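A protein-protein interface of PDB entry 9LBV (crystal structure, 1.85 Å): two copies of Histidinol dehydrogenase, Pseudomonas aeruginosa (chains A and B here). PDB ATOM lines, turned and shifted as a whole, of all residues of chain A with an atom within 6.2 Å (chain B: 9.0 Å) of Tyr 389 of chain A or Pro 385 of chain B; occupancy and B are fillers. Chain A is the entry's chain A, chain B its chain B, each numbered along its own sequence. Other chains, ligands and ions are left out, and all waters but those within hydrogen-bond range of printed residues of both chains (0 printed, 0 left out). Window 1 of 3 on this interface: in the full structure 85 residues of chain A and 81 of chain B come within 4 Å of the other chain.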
ATOM      1  N   GLN A 123     -11.794  41.703  -1.088  1.00  0.00           N
ATOM      2  CA  GLN A 123     -12.497  40.800  -0.192  1.00  0.00           C
ATOM      3  C   GLN A 123     -12.226  41.205   1.236  1.00  0.00           C
ATOM      4  O   GLN A 123     -11.098  41.560   1.575  1.00  0.00           O
ATOM      5  CB  GLN A 123     -12.048  39.353  -0.375  1.00  0.00           C
ATOM      6  CG  GLN A 123     -12.380  38.800  -1.713  1.00  0.00           C
ATOM      7  CD  GLN A 123     -11.997  37.343  -1.807  1.00  0.00           C
ATOM      8  OE1 GLN A 123     -10.848  36.982  -1.558  1.00  0.00           O
ATOM      9  NE2 GLN A 123     -12.954  36.496  -2.168  1.00  0.00           N
ATOM     10  N   ALA A 156      -5.598  30.925  11.226  1.00  0.00           N
ATOM     11  CA  ALA A 156      -6.612  31.787  10.620  1.00  0.00           C
ATOM     12  C   ALA A 156      -7.188  32.803  11.604  1.00  0.00           C
ATOM     13  O   ALA A 156      -7.693  33.855  11.184  1.00  0.00           O
ATOM     14  CB  ALA A 156      -7.752  30.946  10.034  1.00  0.00           C
ATOM     15  N   LYS A 212     -18.095  25.373  11.589  1.00  0.00           N
ATOM     16  CA  LYS A 212     -17.633  24.357  10.660  1.00  0.00           C
ATOM     17  C   LYS A 212     -17.167  23.154  11.456  1.00  0.00           C
ATOM     18  O   LYS A 212     -16.567  23.311  12.517  1.00  0.00           O
ATOM     19  CB  LYS A 212     -16.493  24.882   9.788  1.00  0.00           C
ATOM     20  CG  LYS A 212     -16.125  23.967   8.639  1.00  0.00           C
ATOM     21  CD  LYS A 212     -15.071  24.629   7.741  1.00  0.00           C
ATOM     22  CE  LYS A 212     -14.721  23.763   6.553  1.00  0.00           C
ATOM     23  NZ  LYS A 212     -14.033  24.560   5.525  1.00  0.00           N
ATOM     24  N   GLY A 387      -6.762  24.249   4.123  1.00  0.00           N
ATOM     25  CA  GLY A 387      -5.846  25.060   4.909  1.00  0.00           C
ATOM     26  C   GLY A 387      -6.506  26.246   5.591  1.00  0.00           C
ATOM     27  O   GLY A 387      -7.694  26.201   5.922  1.00  0.00           O
ATOM     28  N   VAL A 388      -5.739  27.321   5.790  1.00  0.00           N
ATOM     29  CA  VAL A 388      -6.255  28.499   6.483  1.00  0.00           C
ATOM     30  C   VAL A 388      -7.518  29.008   5.796  1.00  0.00           C
ATOM     31  O   VAL A 388      -8.489  29.409   6.455  1.00  0.00           O
ATOM     32  CB  VAL A 388      -5.159  29.588   6.550  1.00  0.00           C
ATOM     33  CG1 VAL A 388      -5.717  30.906   7.045  1.00  0.00           C
ATOM     34  CG2 VAL A 388      -3.959  29.129   7.366  1.00  0.00           C
ATOM     35  N   TYR A 389      -7.537  28.972   4.459  1.00  0.00           N
ATOM     36  CA  TYR A 389      -8.702  29.433   3.702  1.00  0.00           C
ATOM     37  C   TYR A 389      -9.993  28.791   4.210  1.00  0.00           C
ATOM     38  O   TYR A 389     -11.027  29.462   4.340  1.00  0.00           O
ATOM     39  CB  TYR A 389      -8.503  29.131   2.200  1.00  0.00           C
ATOM     40  CG  TYR A 389      -9.587  29.688   1.301  1.00  0.00           C
ATOM     41  CD1 TYR A 389     -10.782  29.000   1.105  1.00  0.00           C
ATOM     42  CD2 TYR A 389      -9.413  30.904   0.632  1.00  0.00           C
ATOM     43  CE1 TYR A 389     -11.797  29.529   0.290  1.00  0.00           C
ATOM     44  CE2 TYR A 389     -10.416  31.429  -0.186  1.00  0.00           C
ATOM     45  CZ  TYR A 389     -11.595  30.740  -0.357  1.00  0.00           C
ATOM     46  OH  TYR A 389     -12.579  31.254  -1.169  1.00  0.00           O
ATOM     47  N   ASP A 390      -9.942  27.488   4.522  1.00  0.00           N
ATOM     48  CA  ASP A 390     -11.118  26.733   4.931  1.00  0.00           C
ATOM     49  C   ASP A 390     -11.674  27.162   6.291  1.00  0.00           C
ATOM     50  O   ASP A 390     -12.769  26.719   6.654  1.00  0.00           O
ATOM     51  CB  ASP A 390     -10.778  25.229   4.955  1.00  0.00           C
ATOM     52  CG  ASP A 390     -10.548  24.630   3.540  1.00  0.00           C
ATOM     53  OD1 ASP A 390     -11.404  24.827   2.644  1.00  0.00           O
ATOM     54  OD2 ASP A 390      -9.511  23.940   3.331  1.00  0.00           O
ATOM     55  N   PHE A 391     -10.953  28.000   7.049  1.00  0.00           N
ATOM     56  CA  PHE A 391     -11.416  28.515   8.332  1.00  0.00           C
ATOM     57  C   PHE A 391     -11.673  30.024   8.311  1.00  0.00           C
ATOM     58  O   PHE A 391     -11.707  30.668   9.368  1.00  0.00           O
ATOM     59  CB  PHE A 391     -10.422  28.143   9.427  1.00  0.00           C
ATOM     60  CG  PHE A 391     -10.282  26.658   9.614  1.00  0.00           C
ATOM     61  CD1 PHE A 391     -11.245  25.966  10.330  1.00  0.00           C
ATOM     62  CD2 PHE A 391      -9.229  25.958   9.027  1.00  0.00           C
ATOM     63  CE1 PHE A 391     -11.147  24.594  10.504  1.00  0.00           C
ATOM     64  CE2 PHE A 391      -9.114  24.577   9.186  1.00  0.00           C
ATOM     65  CZ  PHE A 391     -10.082  23.891   9.920  1.00  0.00           C
ATOM     66  N   GLN A 392     -11.895  30.588   7.129  1.00  0.00           N
ATOM     67  CA  GLN A 392     -12.173  32.006   6.966  1.00  0.00           C
ATOM     68  C   GLN A 392     -13.490  32.191   6.223  1.00  0.00           C
ATOM     69  O   GLN A 392     -13.890  31.342   5.424  1.00  0.00           O
ATOM     70  CB  GLN A 392     -11.045  32.707   6.196  1.00  0.00           C
ATOM     71  CG  GLN A 392      -9.653  32.576   6.812  1.00  0.00           C
ATOM     72  CD  GLN A 392      -8.564  33.152   5.889  1.00  0.00           C
ATOM     73  OE1 GLN A 392      -8.470  32.777   4.732  1.00  0.00           O
ATOM     74  NE2 GLN A 392      -7.766  34.079   6.401  1.00  0.00           N
ATOM     75  N   LYS A 393     -14.160  33.305   6.499  1.00  0.00           N
ATOM     76  CA  LYS A 393     -15.331  33.733   5.756  1.00  0.00           C
ATOM     77  C   LYS A 393     -14.905  34.927   4.908  1.00  0.00           C
ATOM     78  O   LYS A 393     -14.092  35.754   5.348  1.00  0.00           O
ATOM     79  CB  LYS A 393     -16.487  34.079   6.720  1.00  0.00           C
ATOM     80  CG  LYS A 393     -17.789  34.626   6.083  1.00  0.00           C
ATOM     81  CD  LYS A 393     -17.730  36.076   5.576  1.00  0.00           C
ATOM     82  CE  LYS A 393     -19.093  36.755   5.603  1.00  0.00           C
ATOM     83  NZ  LYS A 393     -19.949  36.306   4.462  1.00  0.00           N
ATOM     84  N   ARG A 394     -15.437  35.009   3.689  1.00  0.00           N
ATOM     85  CA  ARG A 394     -15.069  36.061   2.748  1.00  0.00           C
ATOM     86  C   ARG A 394     -16.313  36.789   2.263  1.00  0.00           C
ATOM     87  O   ARG A 394     -17.318  36.154   1.929  1.00  0.00           O
ATOM     88  CB  ARG A 394     -14.305  35.490   1.552  1.00  0.00           C
ATOM     89  CG  ARG A 394     -12.970  34.933   1.947  1.00  0.00           C
ATOM     90  CD  ARG A 394     -12.182  34.357   0.796  1.00  0.00           C
ATOM     91  NE  ARG A 394     -10.775  34.725   0.929  1.00  0.00           N
ATOM     92  CZ  ARG A 394      -9.964  34.229   1.854  1.00  0.00           C
ATOM     93  NH1 ARG A 394     -10.400  33.378   2.772  1.00  0.00           N
ATOM     94  NH2 ARG A 394      -8.688  34.608   1.868  1.00  0.00           N
ATOM     95  N   TYR B 102      -9.506  36.234 -17.038  1.00  0.00           N
ATOM     96  CA  TYR B 102      -9.236  36.092 -15.614  1.00  0.00           C
ATOM     97  C   TYR B 102      -8.946  34.641 -15.262  1.00  0.00           C
ATOM     98  O   TYR B 102      -7.943  34.337 -14.616  1.00  0.00           O
ATOM     99  CB  TYR B 102     -10.438  36.636 -14.838  1.00  0.00           C
ATOM    100  CG  TYR B 102     -10.501  36.356 -13.354  1.00  0.00           C
ATOM    101  CD1 TYR B 102     -11.124  35.208 -12.871  1.00  0.00           C
ATOM    102  CD2 TYR B 102      -9.999  37.273 -12.427  1.00  0.00           C
ATOM    103  CE1 TYR B 102     -11.208  34.953 -11.514  1.00  0.00           C
ATOM    104  CE2 TYR B 102     -10.086  37.035 -11.081  1.00  0.00           C
ATOM    105  CZ  TYR B 102     -10.695  35.868 -10.624  1.00  0.00           C
ATOM    106  OH  TYR B 102     -10.792  35.607  -9.273  1.00  0.00           O
ATOM    107  N   HIS B 103      -9.800  33.717 -15.717  1.00  0.00           N
ATOM    108  CA  HIS B 103      -9.609  32.310 -15.354  1.00  0.00           C
ATOM    109  C   HIS B 103      -8.339  31.727 -15.965  1.00  0.00           C
ATOM    110  O   HIS B 103      -7.693  30.871 -15.351  1.00  0.00           O
ATOM    111  CB  HIS B 103     -10.842  31.495 -15.758  1.00  0.00           C
ATOM    112  CG  HIS B 103     -12.011  31.738 -14.861  1.00  0.00           C
ATOM    113  ND1 HIS B 103     -11.932  31.578 -13.492  1.00  0.00           N
ATOM    114  CD2 HIS B 103     -13.261  32.188 -15.118  1.00  0.00           C
ATOM    115  CE1 HIS B 103     -13.096  31.890 -12.947  1.00  0.00           C
ATOM    116  NE2 HIS B 103     -13.919  32.266 -13.911  1.00  0.00           N
ATOM    117  N   GLN B 106      -5.602  32.535 -13.627  1.00  0.00           N
ATOM    118  CA  GLN B 106      -5.680  31.827 -12.359  1.00  0.00           C
ATOM    119  C   GLN B 106      -5.332  30.347 -12.474  1.00  0.00           C
ATOM    120  O   GLN B 106      -5.001  29.722 -11.459  1.00  0.00           O
ATOM    121  CB  GLN B 106      -7.089  31.975 -11.772  1.00  0.00           C
ATOM    122  CG  GLN B 106      -7.427  33.421 -11.453  1.00  0.00           C
ATOM    123  CD  GLN B 106      -8.085  33.583 -10.092  1.00  0.00           C
ATOM    124  OE1 GLN B 106      -7.658  34.401  -9.271  1.00  0.00           O
ATOM    125  NE2 GLN B 106      -9.137  32.794  -9.844  1.00  0.00           N
ATOM    126  N   GLN B 108      -3.888  26.844 -12.506  1.00  0.00           N
ATOM    127  CA  GLN B 108      -2.655  26.227 -12.035  1.00  0.00           C
ATOM    128  C   GLN B 108      -2.626  24.763 -12.455  1.00  0.00           C
ATOM    129  O   GLN B 108      -3.668  24.121 -12.609  1.00  0.00           O
ATOM    130  CB  GLN B 108      -2.526  26.327 -10.517  1.00  0.00           C
ATOM    131  CG  GLN B 108      -2.246  27.735  -9.993  1.00  0.00           C
ATOM    132  CD  GLN B 108      -2.184  27.776  -8.476  1.00  0.00           C
ATOM    133  OE1 GLN B 108      -3.054  27.226  -7.792  1.00  0.00           O
ATOM    134  NE2 GLN B 108      -1.146  28.422  -7.941  1.00  0.00           N
ATOM    135  N   PRO B 152     -14.953  28.866 -16.725  1.00  0.00           N
ATOM    136  CA  PRO B 152     -13.906  28.221 -15.910  1.00  0.00           C
ATOM    137  C   PRO B 152     -13.847  26.709 -16.087  1.00  0.00           C
ATOM    138  O   PRO B 152     -12.739  26.149 -16.090  1.00  0.00           O
ATOM    139  CB  PRO B 152     -14.256  28.615 -14.463  1.00  0.00           C
ATOM    140  CG  PRO B 152     -15.642  29.060 -14.499  1.00  0.00           C
ATOM    141  CD  PRO B 152     -15.831  29.691 -15.887  1.00  0.00           C
ATOM    142  N   LYS B 212     -19.649  17.337 -10.825  1.00  0.00           N
ATOM    143  CA  LYS B 212     -19.996  18.501 -10.022  1.00  0.00           C
ATOM    144  C   LYS B 212     -21.198  19.175 -10.657  1.00  0.00           C
ATOM    145  O   LYS B 212     -21.287  19.259 -11.888  1.00  0.00           O
ATOM    146  CB  LYS B 212     -18.815  19.474  -9.926  1.00  0.00           C
ATOM    147  CG  LYS B 212     -19.020  20.595  -8.927  1.00  0.00           C
ATOM    148  CD  LYS B 212     -17.912  21.629  -9.032  1.00  0.00           C
ATOM    149  CE  LYS B 212     -18.024  22.629  -7.918  1.00  0.00           C
ATOM    150  NZ  LYS B 212     -16.716  22.928  -7.353  1.00  0.00           N
ATOM    151  N   ASP B 235     -21.347  23.415  -5.845  1.00  0.00           N
ATOM    152  CA  ASP B 235     -20.858  24.711  -5.407  1.00  0.00           C
ATOM    153  C   ASP B 235     -21.714  25.207  -4.244  1.00  0.00           C
ATOM    154  O   ASP B 235     -22.613  24.514  -3.766  1.00  0.00           O
ATOM    155  CB  ASP B 235     -20.860  25.716  -6.566  1.00  0.00           C
ATOM    156  CG  ASP B 235     -22.235  25.886  -7.213  1.00  0.00           C
ATOM    157  OD1 ASP B 235     -23.204  25.163  -6.851  1.00  0.00           O
ATOM    158  OD2 ASP B 235     -22.339  26.752  -8.111  1.00  0.00           O
ATOM    159  N   MET B 236     -21.429  26.428  -3.791  1.00  0.00           N
ATOM    160  CA  MET B 236     -22.270  27.116  -2.818  1.00  0.00           C
ATOM    161  C   MET B 236     -23.727  27.048  -3.238  1.00  0.00           C
ATOM    162  O   MET B 236     -24.058  27.285  -4.398  1.00  0.00           O
ATOM    163  CB  MET B 236     -21.842  28.579  -2.717  1.00  0.00           C
ATOM    164  CG  MET B 236     -22.743  29.453  -1.847  1.00  0.00           C
ATOM    165  SD  MET B 236     -21.816  30.812  -1.099  1.00  0.00           S
ATOM    166  CE  MET B 236     -20.181  30.078  -0.941  1.00  0.00           C
ATOM    167  N   ASN B 371     -21.252  36.267  -4.854  1.00  0.00           N
ATOM    168  CA  ASN B 371     -20.184  36.598  -3.896  1.00  0.00           C
ATOM    169  C   ASN B 371     -18.793  36.327  -4.481  1.00  0.00           C
ATOM    170  O   ASN B 371     -17.870  35.928  -3.765  1.00  0.00           O
ATOM    171  CB  ASN B 371     -20.369  35.849  -2.567  1.00  0.00           C
ATOM    172  CG  ASN B 371     -19.690  36.548  -1.382  1.00  0.00           C
ATOM    173  OD1 ASN B 371     -19.409  37.752  -1.416  1.00  0.00           O
ATOM    174  ND2 ASN B 371     -19.431  35.787  -0.326  1.00  0.00           N
ATOM    175  N   HIS B 372     -18.638  36.531  -5.790  1.00  0.00           N
ATOM    176  CA  HIS B 372     -17.342  36.470  -6.452  1.00  0.00           C
ATOM    177  C   HIS B 372     -16.836  37.886  -6.697  1.00  0.00           C
ATOM    178  O   HIS B 372     -17.621  38.809  -6.940  1.00  0.00           O
ATOM    179  CB  HIS B 372     -17.425  35.740  -7.795  1.00  0.00           C
ATOM    180  CG  HIS B 372     -17.796  34.295  -7.691  1.00  0.00           C
ATOM    181  ND1 HIS B 372     -18.666  33.811  -6.737  1.00  0.00           N
ATOM    182  CD2 HIS B 372     -17.443  33.232  -8.451  1.00  0.00           C
ATOM    183  CE1 HIS B 372     -18.818  32.510  -6.901  1.00  0.00           C
ATOM    184  NE2 HIS B 372     -18.087  32.133  -7.934  1.00  0.00           N
ATOM    185  N   PHE B 382      -5.127  37.458  -6.792  1.00  0.00           N
ATOM    186  CA  PHE B 382      -5.545  36.901  -5.505  1.00  0.00           C
ATOM    187  C   PHE B 382      -6.197  35.541  -5.719  1.00  0.00           C
ATOM    188  O   PHE B 382      -7.274  35.442  -6.325  1.00  0.00           O
ATOM    189  CB  PHE B 382      -6.477  37.870  -4.788  1.00  0.00           C
ATOM    190  CG  PHE B 382      -5.809  39.160  -4.447  1.00  0.00           C
ATOM    191  CD1 PHE B 382      -5.770  40.194  -5.367  1.00  0.00           C
ATOM    192  CD2 PHE B 382      -5.159  39.317  -3.229  1.00  0.00           C
ATOM    193  CE1 PHE B 382      -5.119  41.381  -5.065  1.00  0.00           C
ATOM    194  CE2 PHE B 382      -4.506  40.505  -2.923  1.00  0.00           C
ATOM    195  CZ  PHE B 382      -4.486  41.533  -3.840  1.00  0.00           C
ATOM    196  N   SER B 383      -5.546  34.499  -5.201  1.00  0.00           N
ATOM    197  CA  SER B 383      -5.950  33.125  -5.445  1.00  0.00           C
ATOM    198  C   SER B 383      -7.299  32.823  -4.805  1.00  0.00           C
ATOM    199  O   SER B 383      -7.703  33.426  -3.807  1.00  0.00           O
ATOM    200  CB  SER B 383      -4.898  32.152  -4.911  1.00  0.00           C
ATOM    201  OG  SER B 383      -3.929  31.859  -5.905  1.00  0.00           O
ATOM    202  N   SER B 384      -7.989  31.850  -5.394  1.00  0.00           N
ATOM    203  CA  SER B 384      -9.283  31.443  -4.913  1.00  0.00           C
ATOM    204  C   SER B 384      -9.494  29.988  -5.306  1.00  0.00           C
ATOM    205  O   SER B 384      -9.123  29.603  -6.426  1.00  0.00           O
ATOM    206  CB  SER B 384     -10.387  32.331  -5.506  1.00  0.00           C
ATOM    207  OG  SER B 384     -11.678  31.839  -5.192  1.00  0.00           O
ATOM    208  N   PRO B 385     -10.041  29.154  -4.415  1.00  0.00           N
ATOM    209  CA  PRO B 385     -10.467  27.807  -4.828  1.00  0.00           C
ATOM    210  C   PRO B 385     -11.753  27.805  -5.636  1.00  0.00           C
ATOM    211  O   PRO B 385     -12.196  26.734  -6.065  1.00  0.00           O
ATOM    212  CB  PRO B 385     -10.658  27.070  -3.496  1.00  0.00           C
ATOM    213  CG  PRO B 385     -10.925  28.140  -2.527  1.00  0.00           C
ATOM    214  CD  PRO B 385     -10.104  29.326  -2.957  1.00  0.00           C
ATOM    215  N   LEU B 386     -12.387  28.955  -5.824  1.00  0.00           N
ATOM    216  CA  LEU B 386     -13.457  29.058  -6.798  1.00  0.00           C
ATOM    217  C   LEU B 386     -12.850  29.211  -8.188  1.00  0.00           C
ATOM    218  O   LEU B 386     -11.636  29.369  -8.350  1.00  0.00           O
ATOM    219  CB  LEU B 386     -14.364  30.247  -6.479  1.00  0.00           C
ATOM    220  CG  LEU B 386     -14.650  30.500  -5.001  1.00  0.00           C
ATOM    221  CD1 LEU B 386     -14.983  31.973  -4.748  1.00  0.00           C
ATOM    222  CD2 LEU B 386     -15.769  29.584  -4.538  1.00  0.00           C
ATOM    223  N   GLY B 387     -13.698  29.172  -9.203  1.00  0.00           N
ATOM    224  CA  GLY B 387     -13.164  29.367 -10.529  1.00  0.00           C
ATOM    225  C   GLY B 387     -12.569  28.084 -11.057  1.00  0.00           C
ATOM    226  O   GLY B 387     -13.144  27.016 -10.843  1.00  0.00           O
ATOM    227  N   VAL B 388     -11.427  28.177 -11.745  1.00  0.00           N
ATOM    228  CA  VAL B 388     -10.837  27.003 -12.386  1.00  0.00           C
ATOM    229  C   VAL B 388     -10.560  25.900 -11.362  1.00  0.00           C
ATOM    230  O   VAL B 388     -10.736  24.714 -11.656  1.00  0.00           O
ATOM    231  CB  VAL B 388      -9.573  27.411 -13.166  1.00  0.00           C
ATOM    232  CG1 VAL B 388      -8.841  26.187 -13.711  1.00  0.00           C
ATOM    233  CG2 VAL B 388      -9.960  28.327 -14.321  1.00  0.00           C
ATOM    234  N   TYR B 389     -10.150  26.265 -10.142  1.00  0.00           N
ATOM    235  CA  TYR B 389      -9.943  25.293  -9.058  1.00  0.00           C
ATOM    236  C   TYR B 389     -11.178  24.432  -8.794  1.00  0.00           C
ATOM    237  O   TYR B 389     -11.049  23.256  -8.436  1.00  0.00           O
ATOM    238  CB  TYR B 389      -9.542  26.025  -7.770  1.00  0.00           C
ATOM    239  CG  TYR B 389      -8.916  25.153  -6.689  1.00  0.00           C
ATOM    240  CD1 TYR B 389      -9.724  24.494  -5.764  1.00  0.00           C
ATOM    241  CD2 TYR B 389      -7.528  25.044  -6.546  1.00  0.00           C
ATOM    242  CE1 TYR B 389      -9.183  23.712  -4.758  1.00  0.00           C
ATOM    243  CE2 TYR B 389      -6.971  24.263  -5.523  1.00  0.00           C
ATOM    244  CZ  TYR B 389      -7.811  23.598  -4.635  1.00  0.00           C
ATOM    245  OH  TYR B 389      -7.301  22.816  -3.613  1.00  0.00           O
ATOM    246  N   ASP B 390     -12.377  25.023  -8.924  1.00  0.00           N
ATOM    247  CA  ASP B 390     -13.669  24.340  -8.802  1.00  0.00           C
ATOM    248  C   ASP B 390     -13.723  23.050  -9.566  1.00  0.00           C
ATOM    249  O   ASP B 390     -14.327  22.071  -9.131  1.00  0.00           O
ATOM    250  CB  ASP B 390     -14.797  25.190  -9.413  1.00  0.00           C
ATOM    251  CG  ASP B 390     -15.310  26.293  -8.505  1.00  0.00           C
ATOM    252  OD1 ASP B 390     -15.682  25.992  -7.340  1.00  0.00           O
ATOM    253  OD2 ASP B 390     -15.387  27.455  -8.987  1.00  0.00           O
ATOM    254  N   PHE B 391     -13.268  23.120 -10.810  1.00  0.00           N
ATOM    255  CA  PHE B 391     -13.480  22.079 -11.799  1.00  0.00           C
ATOM    256  C   PHE B 391     -12.246  21.228 -11.996  1.00  0.00           C
ATOM    257  O   PHE B 391     -12.113  20.573 -13.027  1.00  0.00           O
ATOM    258  CB  PHE B 391     -13.947  22.713 -13.108  1.00  0.00           C
ATOM    259  CG  PHE B 391     -15.177  23.549 -12.959  1.00  0.00           C
ATOM    260  CD1 PHE B 391     -16.429  22.946 -13.000  1.00  0.00           C
ATOM    261  CD2 PHE B 391     -15.103  24.917 -12.792  1.00  0.00           C
ATOM    262  CE1 PHE B 391     -17.593  23.694 -12.882  1.00  0.00           C
ATOM    263  CE2 PHE B 391     -16.278  25.681 -12.660  1.00  0.00           C
ATOM    264  CZ  PHE B 391     -17.519  25.060 -12.696  1.00  0.00           C
ATOM    265  N   GLN B 392     -11.352  21.216 -11.018  1.00  0.00           N
ATOM    266  CA  GLN B 392     -10.134  20.425 -11.089  1.00  0.00           C
ATOM    267  C   GLN B 392     -10.069  19.471  -9.904  1.00  0.00           C
ATOM    268  O   GLN B 392     -10.640  19.727  -8.848  1.00  0.00           O
ATOM    269  CB  GLN B 392      -8.882  21.315 -11.084  1.00  0.00           C
ATOM    270  CG  GLN B 392      -8.653  22.135 -12.350  1.00  0.00           C
ATOM    271  CD  GLN B 392      -7.456  23.057 -12.182  1.00  0.00           C
ATOM    272  OE1 GLN B 392      -7.266  23.617 -11.113  1.00  0.00           O
ATOM    273  NE2 GLN B 392      -6.638  23.204 -13.228  1.00  0.00           N
ATOM    274  N   ARG B 394      -7.186  17.532  -7.439  1.00  0.00           N
ATOM    275  CA  ARG B 394      -5.799  17.643  -7.004  1.00  0.00           C
ATOM    276  C   ARG B 394      -5.394  16.395  -6.235  1.00  0.00           C
ATOM    277  O   ARG B 394      -5.994  16.077  -5.204  1.00  0.00           O
ATOM    278  CB  ARG B 394      -5.608  18.877  -6.130  1.00  0.00           C
ATOM    279  CG  ARG B 394      -5.023  20.033  -6.879  1.00  0.00           C
ATOM    280  CD  ARG B 394      -5.598  21.325  -6.404  1.00  0.00           C
ATOM    281  NE  ARG B 394      -5.507  22.307  -7.479  1.00  0.00           N
ATOM    282  CZ  ARG B 394      -4.442  23.061  -7.718  1.00  0.00           C
ATOM    283  NH1 ARG B 394      -3.409  23.087  -6.882  1.00  0.00           N
ATOM    284  NH2 ARG B 394      -4.418  23.816  -8.816  1.00  0.00           N
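O of Arg 394 of chain A lies within hydrogen-bond range of ND2 of Asn 371 of chain B (3.1 Å).
The side-chain amide oxygen (OE1) of Gln 123 of chain A is in hydrogen-bond range of the guanidinium group (NE) of Arg 394 of chain A (3.4 Å). The side-chain amide oxygen (OE1) of Gln 392 of chain A lies within hydrogen-bond range of the guanidinium group (NH1) of Arg 394 of chain A, at 2.8 Å. O of Pro 385 of chain B is in hydrogen-bond range of N of Asp 390 of chain B (3.3 Å).
Among the printed residues, pairs that only touch across the chains: Tyr 389 of chain A with Pro 385 of chain B (3.3 Å).
Tyr 389 of chain A touches one residue of chain B. Pro 385 of chain B touches just one residue of chain A: Tyr 389 (3.3 Å). Gly 387 of chain A touches none of the printed residues of chain B. No residue of chain B comes within 4 Å of Val 388 of chain A. Of the printed residues of chain A, Asn 371 of chain B touches Arg 394. Printed residues of chain B within 4 Å of Arg 394 of chain A: Asn 371. Lys 393 of chain A touches none of the printed residues of chain B. Tyr 389 of chain B touches none of the printed residues of chain A. The nearest residue of chain B that does not touch Tyr 389 of chain A is Ser 384 of chain B (4.2 Å). The nearest printed residue of chain B that does not touch Arg 394 of chain A is Ser 383 of chain B (5.8 Å).
Of the 11 printed residues of chain A, 2 touch a printed residue of chain B. Hydrophobic or aromatic side chains of chain A that line the printed part of chain B: Tyr 389. Along chain A the printed residues that touch a printed residue of chain B span positions 389 to 394. Among the printed residues, 2 pairs touch across the chains.
Positions printed for both chains: 212, 387, 388, 389, 390, 391, 392 and 394. Of the 2 pairs that touch across the chains among the printed residues, none has its exchanged pair printed and touching as well.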
